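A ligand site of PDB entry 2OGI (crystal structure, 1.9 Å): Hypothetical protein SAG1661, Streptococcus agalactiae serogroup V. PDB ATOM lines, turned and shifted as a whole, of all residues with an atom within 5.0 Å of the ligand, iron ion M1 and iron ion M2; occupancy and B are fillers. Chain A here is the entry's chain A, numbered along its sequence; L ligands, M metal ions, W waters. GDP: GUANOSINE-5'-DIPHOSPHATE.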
ATOM      1  N   HIS A  30      22.730  41.836 -15.053  1.00  0.00           N
ATOM      2  CA  HIS A  30      22.317  40.902 -14.044  1.00  0.00           C
ATOM      3  C   HIS A  30      22.303  41.569 -12.695  1.00  0.00           C
ATOM      4  O   HIS A  30      21.364  41.432 -11.917  1.00  0.00           O
ATOM      5  CB  HIS A  30      23.228  39.702 -14.036  1.00  0.00           C
ATOM      6  CG  HIS A  30      23.198  38.917 -12.761  1.00  0.00           C
ATOM      7  ND1 HIS A  30      22.118  38.160 -12.410  1.00  0.00           N
ATOM      8  CD2 HIS A  30      24.115  38.765 -11.785  1.00  0.00           C
ATOM      9  CE1 HIS A  30      22.369  37.555 -11.247  1.00  0.00           C
ATOM     10  NE2 HIS A  30      23.598  37.878 -10.874  1.00  0.00           N
ATOM     11  N   VAL A  34      19.298  42.043 -10.147  1.00  0.00           N
ATOM     12  CA  VAL A  34      19.314  41.631  -8.761  1.00  0.00           C
ATOM     13  C   VAL A  34      19.013  42.774  -7.795  1.00  0.00           C
ATOM     14  O   VAL A  34      18.310  42.594  -6.810  1.00  0.00           O
ATOM     15  CB  VAL A  34      20.661  40.941  -8.384  1.00  0.00           C
ATOM     16  CG1 VAL A  34      20.644  40.518  -6.900  1.00  0.00           C
ATOM     17  CG2 VAL A  34      20.861  39.715  -9.236  1.00  0.00           C
ATOM     18  N   HIS A  59      26.929  42.328  -5.005  1.00  0.00           N
ATOM     19  CA  HIS A  59      27.111  40.895  -4.644  1.00  0.00           C
ATOM     20  C   HIS A  59      28.099  40.162  -5.545  1.00  0.00           C
ATOM     21  O   HIS A  59      28.837  39.319  -5.089  1.00  0.00           O
ATOM     22  CB  HIS A  59      25.754  40.174  -4.543  1.00  0.00           C
ATOM     23  CG  HIS A  59      25.206  39.762  -5.842  1.00  0.00           C
ATOM     24  ND1 HIS A  59      24.650  40.645  -6.736  1.00  0.00           N
ATOM     25  CD2 HIS A  59      25.209  38.567  -6.457  1.00  0.00           C
ATOM     26  CE1 HIS A  59      24.315  39.998  -7.838  1.00  0.00           C
ATOM     27  NE2 HIS A  59      24.666  38.734  -7.708  1.00  0.00           N
ATOM     28  N   ASP A  60      28.110  40.519  -6.819  1.00  0.00           N
ATOM     29  CA  ASP A  60      28.983  39.954  -7.839  1.00  0.00           C
ATOM     30  C   ASP A  60      30.105  40.888  -8.228  1.00  0.00           C
ATOM     31  O   ASP A  60      30.596  40.803  -9.296  1.00  0.00           O
ATOM     32  CB  ASP A  60      28.142  39.598  -9.067  1.00  0.00           C
ATOM     33  CG  ASP A  60      27.596  38.146  -8.997  1.00  0.00           C
ATOM     34  OD1 ASP A  60      28.055  37.349  -8.120  1.00  0.00           O
ATOM     35  OD2 ASP A  60      26.691  37.815  -9.800  1.00  0.00           O
ATOM     36  N   LYS A  63      33.052  38.877  -9.469  1.00  0.00           N
ATOM     37  CA  LYS A  63      32.723  37.725 -10.278  1.00  0.00           C
ATOM     38  C   LYS A  63      33.768  37.430 -11.357  1.00  0.00           C
ATOM     39  O   LYS A  63      34.011  36.285 -11.666  1.00  0.00           O
ATOM     40  CB  LYS A  63      31.356  37.930 -10.924  1.00  0.00           C
ATOM     41  CG  LYS A  63      30.792  36.796 -11.769  1.00  0.00           C
ATOM     42  CD  LYS A  63      30.563  35.476 -11.046  1.00  0.00           C
ATOM     43  CE  LYS A  63      29.671  34.614 -11.915  1.00  0.00           C
ATOM     44  NZ  LYS A  63      29.451  33.233 -11.462  1.00  0.00           N
ATOM     45  N   TRP A  86      38.995  25.040  -4.562  1.00  0.00           N
ATOM     46  CA  TRP A  86      37.741  25.301  -5.200  1.00  0.00           C
ATOM     47  C   TRP A  86      38.010  26.245  -6.369  1.00  0.00           C
ATOM     48  O   TRP A  86      39.027  26.132  -7.061  1.00  0.00           O
ATOM     49  CB  TRP A  86      36.694  25.789  -4.202  1.00  0.00           C
ATOM     50  CG  TRP A  86      36.384  24.755  -3.176  1.00  0.00           C
ATOM     51  CD1 TRP A  86      37.062  24.524  -2.045  1.00  0.00           C
ATOM     52  CD2 TRP A  86      35.342  23.781  -3.222  1.00  0.00           C
ATOM     53  NE1 TRP A  86      36.504  23.475  -1.347  1.00  0.00           N
ATOM     54  CE2 TRP A  86      35.439  23.007  -2.049  1.00  0.00           C
ATOM     55  CE3 TRP A  86      34.289  23.524  -4.115  1.00  0.00           C
ATOM     56  CZ2 TRP A  86      34.558  21.950  -1.763  1.00  0.00           C
ATOM     57  CZ3 TRP A  86      33.404  22.457  -3.829  1.00  0.00           C
ATOM     58  CH2 TRP A  86      33.556  21.686  -2.672  1.00  0.00           C
ATOM     59  N   ASN A  89      33.402  30.017  -8.458  1.00  0.00           N
ATOM     60  CA  ASN A  89      32.023  29.921  -8.011  1.00  0.00           C
ATOM     61  C   ASN A  89      31.976  30.152  -6.512  1.00  0.00           C
ATOM     62  O   ASN A  89      31.116  30.848  -5.943  1.00  0.00           O
ATOM     63  CB  ASN A  89      31.417  28.527  -8.306  1.00  0.00           C
ATOM     64  CG  ASN A  89      31.045  28.321  -9.744  1.00  0.00           C
ATOM     65  OD1 ASN A  89      31.093  29.250 -10.567  1.00  0.00           O
ATOM     66  ND2 ASN A  89      30.712  27.067 -10.081  1.00  0.00           N
ATOM     67  N   ILE A  90      32.946  29.565  -5.841  1.00  0.00           N
ATOM     68  CA  ILE A  90      33.006  29.634  -4.394  1.00  0.00           C
ATOM     69  C   ILE A  90      33.695  30.923  -3.972  1.00  0.00           C
ATOM     70  O   ILE A  90      33.319  31.541  -2.989  1.00  0.00           O
ATOM     71  CB  ILE A  90      33.791  28.393  -3.833  1.00  0.00           C
ATOM     72  CG1 ILE A  90      33.029  27.083  -4.069  1.00  0.00           C
ATOM     73  CG2 ILE A  90      34.107  28.533  -2.378  1.00  0.00           C
ATOM     74  CD1 ILE A  90      31.582  27.185  -3.948  1.00  0.00           C
ATOM     75  N   HIS A  92      34.125  33.964  -5.482  1.00  0.00           N
ATOM     76  CA  HIS A  92      33.792  35.364  -5.812  1.00  0.00           C
ATOM     77  C   HIS A  92      32.988  36.074  -4.768  1.00  0.00           C
ATOM     78  O   HIS A  92      33.081  37.310  -4.728  1.00  0.00           O
ATOM     79  CB  HIS A  92      33.203  35.518  -7.237  1.00  0.00           C
ATOM     80  CG  HIS A  92      31.785  35.033  -7.372  1.00  0.00           C
ATOM     81  ND1 HIS A  92      31.486  33.700  -7.526  1.00  0.00           N
ATOM     82  CD2 HIS A  92      30.597  35.692  -7.296  1.00  0.00           C
ATOM     83  CE1 HIS A  92      30.158  33.553  -7.586  1.00  0.00           C
ATOM     84  NE2 HIS A  92      29.603  34.745  -7.439  1.00  0.00           N
ATOM     85  N   HIS A 118      26.382  34.654  -0.643  1.00  0.00           N
ATOM     86  CA  HIS A 118      25.330  34.716  -1.658  1.00  0.00           C
ATOM     87  C   HIS A 118      25.243  33.483  -2.540  1.00  0.00           C
ATOM     88  O   HIS A 118      24.175  33.202  -3.033  1.00  0.00           O
ATOM     89  CB  HIS A 118      25.406  35.996  -2.521  1.00  0.00           C
ATOM     90  CG  HIS A 118      26.353  35.925  -3.679  1.00  0.00           C
ATOM     91  ND1 HIS A 118      27.645  36.401  -3.603  1.00  0.00           N
ATOM     92  CD2 HIS A 118      26.170  35.589  -4.983  1.00  0.00           C
ATOM     93  CE1 HIS A 118      28.223  36.299  -4.785  1.00  0.00           C
ATOM     94  NE2 HIS A 118      27.356  35.819  -5.644  1.00  0.00           N
ATOM     95  N   THR A 119      26.327  32.745  -2.722  1.00  0.00           N
ATOM     96  CA  THR A 119      26.335  31.596  -3.618  1.00  0.00           C
ATOM     97  C   THR A 119      25.933  30.335  -2.858  1.00  0.00           C
ATOM     98  O   THR A 119      25.136  29.559  -3.309  1.00  0.00           O
ATOM     99  CB  THR A 119      27.735  31.404  -4.283  1.00  0.00           C
ATOM    100  OG1 THR A 119      28.202  32.660  -4.779  1.00  0.00           O
ATOM    101  CG2 THR A 119      27.697  30.327  -5.383  1.00  0.00           C
ATOM    102  N   VAL A 120      26.431  30.153  -1.640  1.00  0.00           N
ATOM    103  CA  VAL A 120      26.289  28.898  -0.921  1.00  0.00           C
ATOM    104  C   VAL A 120      25.311  28.915   0.254  1.00  0.00           C
ATOM    105  O   VAL A 120      24.857  27.868   0.700  1.00  0.00           O
ATOM    106  CB  VAL A 120      27.675  28.436  -0.433  1.00  0.00           C
ATOM    107  CG1 VAL A 120      28.532  28.186  -1.636  1.00  0.00           C
ATOM    108  CG2 VAL A 120      28.342  29.440   0.409  1.00  0.00           C
ATOM    109  N   ASP A 136      19.153  36.982  -6.443  1.00  0.00           N
ATOM    110  CA  ASP A 136      20.165  36.548  -7.424  1.00  0.00           C
ATOM    111  C   ASP A 136      19.643  35.508  -8.407  1.00  0.00           C
ATOM    112  O   ASP A 136      20.025  35.483  -9.583  1.00  0.00           O
ATOM    113  CB  ASP A 136      21.365  35.975  -6.647  1.00  0.00           C
ATOM    114  CG  ASP A 136      22.571  35.726  -7.535  1.00  0.00           C
ATOM    115  OD1 ASP A 136      22.769  36.501  -8.518  1.00  0.00           O
ATOM    116  OD2 ASP A 136      23.269  34.722  -7.292  1.00  0.00           O
ATOM    117  N   ARG A 142      17.071  36.396 -15.714  1.00  0.00           N
ATOM    118  CA  ARG A 142      17.252  34.937 -15.614  1.00  0.00           C
ATOM    119  C   ARG A 142      16.152  34.175 -16.357  1.00  0.00           C
ATOM    120  O   ARG A 142      15.002  34.568 -16.318  1.00  0.00           O
ATOM    121  CB  ARG A 142      17.243  34.437 -14.169  1.00  0.00           C
ATOM    122  CG  ARG A 142      18.316  34.973 -13.246  1.00  0.00           C
ATOM    123  CD  ARG A 142      19.672  34.365 -13.491  1.00  0.00           C
ATOM    124  NE  ARG A 142      20.376  34.238 -12.219  1.00  0.00           N
ATOM    125  CZ  ARG A 142      21.696  34.259 -12.059  1.00  0.00           C
ATOM    126  NH1 ARG A 142      22.504  34.425 -13.097  1.00  0.00           N
ATOM    127  NH2 ARG A 142      22.226  34.140 -10.829  1.00  0.00           N
ATOM    128  N   THR A 169      19.832  23.672  -6.971  1.00  0.00           N
ATOM    129  CA  THR A 169      21.234  23.842  -7.247  1.00  0.00           C
ATOM    130  C   THR A 169      21.963  22.519  -6.899  1.00  0.00           C
ATOM    131  O   THR A 169      22.822  22.100  -7.600  1.00  0.00           O
ATOM    132  CB  THR A 169      21.803  25.017  -6.432  1.00  0.00           C
ATOM    133  OG1 THR A 169      21.162  26.238  -6.873  1.00  0.00           O
ATOM    134  CG2 THR A 169      23.287  25.092  -6.521  1.00  0.00           C
ATOM    135  N   PHE A 172      21.269  20.068  -9.601  1.00  0.00           N
ATOM    136  CA  PHE A 172      21.975  20.452 -10.837  1.00  0.00           C
ATOM    137  C   PHE A 172      23.462  20.037 -10.804  1.00  0.00           C
ATOM    138  O   PHE A 172      24.002  19.500 -11.766  1.00  0.00           O
ATOM    139  CB  PHE A 172      21.830  21.964 -11.035  1.00  0.00           C
ATOM    140  CG  PHE A 172      22.754  22.533 -12.057  1.00  0.00           C
ATOM    141  CD1 PHE A 172      22.490  22.416 -13.398  1.00  0.00           C
ATOM    142  CD2 PHE A 172      23.938  23.157 -11.679  1.00  0.00           C
ATOM    143  CE1 PHE A 172      23.346  22.923 -14.344  1.00  0.00           C
ATOM    144  CE2 PHE A 172      24.800  23.651 -12.625  1.00  0.00           C
ATOM    145  CZ  PHE A 172      24.493  23.537 -13.948  1.00  0.00           C
ATOM    146  N   LEU A 173      24.114  20.312  -9.688  1.00  0.00           N
ATOM    147  CA  LEU A 173      25.528  20.025  -9.509  1.00  0.00           C
ATOM    148  C   LEU A 173      25.764  18.517  -9.526  1.00  0.00           C
ATOM    149  O   LEU A 173      26.722  18.042 -10.099  1.00  0.00           O
ATOM    150  CB  LEU A 173      25.992  20.602  -8.157  1.00  0.00           C
ATOM    151  CG  LEU A 173      26.070  22.149  -8.039  1.00  0.00           C
ATOM    152  CD1 LEU A 173      26.368  22.538  -6.598  1.00  0.00           C
ATOM    153  CD2 LEU A 173      27.112  22.708  -8.973  1.00  0.00           C
ATOM    154  N   GLN A 178      29.678  17.582 -10.225  1.00  0.00           N
ATOM    155  CA  GLN A 178      30.535  18.708  -9.831  1.00  0.00           C
ATOM    156  C   GLN A 178      30.567  18.797  -8.346  1.00  0.00           C
ATOM    157  O   GLN A 178      29.587  18.486  -7.680  1.00  0.00           O
ATOM    158  CB  GLN A 178      29.969  20.043 -10.328  1.00  0.00           C
ATOM    159  CG  GLN A 178      29.860  20.160 -11.829  1.00  0.00           C
ATOM    160  CD  GLN A 178      31.182  20.048 -12.490  1.00  0.00           C
ATOM    161  OE1 GLN A 178      32.140  20.727 -12.097  1.00  0.00           O
ATOM    162  NE2 GLN A 178      31.273  19.179 -13.502  1.00  0.00           N
ATOM    163  N   PRO A 179      31.701  19.245  -7.809  1.00  0.00           N
ATOM    164  CA  PRO A 179      31.746  19.245  -6.343  1.00  0.00           C
ATOM    165  C   PRO A 179      30.755  20.186  -5.744  1.00  0.00           C
ATOM    166  O   PRO A 179      30.406  21.204  -6.354  1.00  0.00           O
ATOM    167  CB  PRO A 179      33.206  19.616  -6.004  1.00  0.00           C
ATOM    168  CG  PRO A 179      33.751  20.213  -7.222  1.00  0.00           C
ATOM    169  CD  PRO A 179      32.945  19.750  -8.418  1.00  0.00           C
ATOM    170  N   ILE A 180      30.294  19.793  -4.561  1.00  0.00           N
ATOM    171  CA  ILE A 180      29.290  20.472  -3.851  1.00  0.00           C
ATOM    172  C   ILE A 180      29.948  20.953  -2.565  1.00  0.00           C
ATOM    173  O   ILE A 180      30.429  20.171  -1.777  1.00  0.00           O
ATOM    174  CB  ILE A 180      28.077  19.529  -3.558  1.00  0.00           C
ATOM    175  CG1 ILE A 180      27.351  19.188  -4.849  1.00  0.00           C
ATOM    176  CG2 ILE A 180      27.150  20.133  -2.502  1.00  0.00           C
ATOM    177  CD1 ILE A 180      26.374  18.040  -4.710  1.00  0.00           C
ATOM    178  N   TYR A 181      29.990  22.278  -2.419  1.00  0.00           N
ATOM    179  CA  TYR A 181      30.577  22.923  -1.279  1.00  0.00           C
ATOM    180  C   TYR A 181      29.810  22.540  -0.087  1.00  0.00           C
ATOM    181  O   TYR A 181      28.611  22.497  -0.119  1.00  0.00           O
ATOM    182  CB  TYR A 181      30.628  24.462  -1.424  1.00  0.00           C
ATOM    183  CG  TYR A 181      31.587  25.195  -0.480  1.00  0.00           C
ATOM    184  CD1 TYR A 181      32.968  24.999  -0.574  1.00  0.00           C
ATOM    185  CD2 TYR A 181      31.113  26.079   0.486  1.00  0.00           C
ATOM    186  CE1 TYR A 181      33.849  25.666   0.244  1.00  0.00           C
ATOM    187  CE2 TYR A 181      31.994  26.778   1.315  1.00  0.00           C
ATOM    188  CZ  TYR A 181      33.349  26.560   1.178  1.00  0.00           C
ATOM    189  OH  TYR A 181      34.247  27.210   1.978  1.00  0.00           O
ATOM    190  N   THR A 184      26.836  24.497   1.143  1.00  0.00           N
ATOM    191  CA  THR A 184      25.675  24.339   0.302  1.00  0.00           C
ATOM    192  C   THR A 184      24.720  23.282   0.884  1.00  0.00           C
ATOM    193  O   THR A 184      23.524  23.469   0.871  1.00  0.00           O
ATOM    194  CB  THR A 184      26.106  24.007  -1.120  1.00  0.00           C
ATOM    195  OG1 THR A 184      26.821  25.134  -1.568  1.00  0.00           O
ATOM    196  CG2 THR A 184      24.923  23.763  -2.072  1.00  0.00           C
HETATM  197  PB  GDP L   1      26.012  34.093 -10.339  1.00  0.00           P
HETATM  198  O1B GDP L   1      26.246  33.285 -11.591  1.00  0.00           O
HETATM  199  O2B GDP L   1      27.368  34.570  -9.817  1.00  0.00           O
HETATM  200  O3B GDP L   1      24.996  35.227 -10.554  1.00  0.00           O
HETATM  201  O3A GDP L   1      25.254  33.054  -9.313  1.00  0.00           O
HETATM  202  PA  GDP L   1      25.872  32.384  -7.964  1.00  0.00           P
HETATM  203  O1A GDP L   1      26.929  33.150  -7.194  1.00  0.00           O
HETATM  204  O2A GDP L   1      24.726  31.946  -7.068  1.00  0.00           O
HETATM  205  O5' GDP L   1      26.514  30.947  -8.434  1.00  0.00           O
HETATM  206  C5' GDP L   1      27.426  30.792  -9.503  1.00  0.00           C
HETATM  207  C4' GDP L   1      27.649  29.293  -9.751  1.00  0.00           C
HETATM  208  O4' GDP L   1      28.102  28.703  -8.534  1.00  0.00           O
HETATM  209  C3' GDP L   1      26.439  28.480 -10.231  1.00  0.00           C
HETATM  210  O3' GDP L   1      26.782  27.728 -11.407  1.00  0.00           O
HETATM  211  C2' GDP L   1      26.132  27.507  -9.114  1.00  0.00           C
HETATM  212  O2' GDP L   1      25.704  26.225  -9.588  1.00  0.00           O
HETATM  213  C1' GDP L   1      27.525  27.399  -8.507  1.00  0.00           C
HETATM  214  N9  GDP L   1      27.457  26.796  -7.166  1.00  0.00           N
HETATM  215  C8  GDP L   1      26.588  27.054  -6.204  1.00  0.00           C
HETATM  216  N7  GDP L   1      26.849  26.279  -5.110  1.00  0.00           N
HETATM  217  C5  GDP L   1      27.902  25.480  -5.455  1.00  0.00           C
HETATM  218  C6  GDP L   1      28.645  24.379  -4.827  1.00  0.00           C
HETATM  219  O6  GDP L   1      28.287  24.068  -3.667  1.00  0.00           O
HETATM  220  N1  GDP L   1      29.672  23.798  -5.535  1.00  0.00           N
HETATM  221  C2  GDP L   1      30.001  24.185  -6.828  1.00  0.00           C
HETATM  222  N2  GDP L   1      31.019  23.575  -7.547  1.00  0.00           N
HETATM  223  N3  GDP L   1      29.324  25.200  -7.451  1.00  0.00           N
HETATM  224  C4  GDP L   1      28.312  25.841  -6.812  1.00  0.00           C
HETATM  225 FE    FE M   1      24.759  37.006  -9.186  1.00  0.00          FE
HETATM  226 FE    FE M   2      27.460  35.294  -7.739  1.00  0.00          FE
HETATM  227  O   HOH W   1      21.834  31.973  -8.149  1.00  0.00           O
HETATM  228  O   HOH W   2      30.739  23.621 -10.583  1.00  0.00           O
HETATM  229  O   HOH W   3      28.218  24.889 -11.935  1.00  0.00           O
HETATM  230  O   HOH W   4      24.783  26.907  -3.701  1.00  0.00           O
HETATM  231  O   HOH W   5      25.483  35.740  -7.877  1.00  0.00           O
HETATM  232  O   HOH W   6      22.511  32.443  -4.927  1.00  0.00           O
HETATM  233  O   HOH W   7      28.152  31.196 -13.335  1.00  0.00           O
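NZ of Lys 63 lies within salt-bridge range of O1B of the ligand. The side-chain amide nitrogen of Asn 89 lies close to an oxygen (O4') of the ligand. An oxygen (O6) of the ligand sits at hydrogen-bond distance from the side-chain hydroxyl (OG1) of Thr 184. An oxygen (O6) of the ligand sits at hydrogen-bond distance from the backbone NH (N) of Tyr 181. N2 of the ligand is in hydrogen-bond range of O of Pro 179 (2.7 Å). The guanidinium group (NH2) of Arg 142 lies close to an oxygen (O3B) of the ligand (3.0 Å). OG1 of Thr 119 lies close to O1A of the ligand (2.8 Å).
OD2 of Asp 136 is in salt-bridge range of NH2 of Arg 142 (3.7 Å). The backbone carbonyl oxygen (O) of Leu 173 lies within hydrogen-bond range of the backbone NH (N) of Gln 178. ND1 of His 92 sits at hydrogen-bond distance from O of Asn 89 (3.3 Å). OG1 of Thr 119 lies close to NE2 of His 118 (3.4 Å). O of His 59 lies close to ND1 of His 118 (3.5 Å).
Thr 169 touches the ligand (CG2 to C8, 3.9 Å). Leu 173 touches the ligand (CD1 to C6, 3.4 Å). C of Ile 180 touches O6 of the ligand (3.7 Å). The nearest printed residue that does not touch the ligand is Phe 172 (4.1 Å).
Three residues have an atom within 4 Å of iron ion M2: Asp 60, His 92 and His 118.
Iron ion M1 is bound by water W5, the side-chain carboxylate of Asp 136, the side-chain carboxylate of Asp 60, a ring nitrogen (NE2) of His 30, an oxygen (O3B) of the ligand and a ring nitrogen (NE2) of His 59. Iron ion M1 has six donor atoms within binding distance.
Water W5 binds iron ion M2 (2.0 Å). Iron ion M2 is bound by a ring nitrogen (NE2) of His 118, 2.2 Å away. The side-chain carboxylate (OD1) of Asp 60 binds iron ion M2. An oxygen (O2B) of the ligand is bound to iron ion M2, 2.2 Å away. A ring nitrogen (NE2) of His 92 binds iron ion M2 (2.2 Å). Iron ion M2 is bound by an oxygen (O1A) of the ligand, 2.3 Å away. Iron ion M2 has six donor atoms within binding distance.
Water W5 lies within hydrogen-bond range of the side-chain carboxylate of Asp 136 and an oxygen (O3A) of the ligand. Water W4 lies within hydrogen-bond range of a nitrogen (N7) of the ligand (2.6 Å), the backbone carbonyl oxygen (O) of Thr 119 (2.7 Å) and the side-chain hydroxyl (OG1) of Thr 184 (3.4 Å). Water W2 lies within hydrogen-bond range of N2 of the ligand and ND2 of Asn 89. Water W1 lies within hydrogen-bond range of O2A of the ligand, OD2 of Asp 136 and NH2 of Arg 142. Water W6 lies within hydrogen-bond range of the backbone carbonyl oxygen of His 118, an oxygen (O2A) of the ligand and the side-chain carboxylate of Asp 136. Water W7 lies within hydrogen-bond range of the side-chain amino group (NZ) of Lys 63 and an oxygen (O1B) of the ligand.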
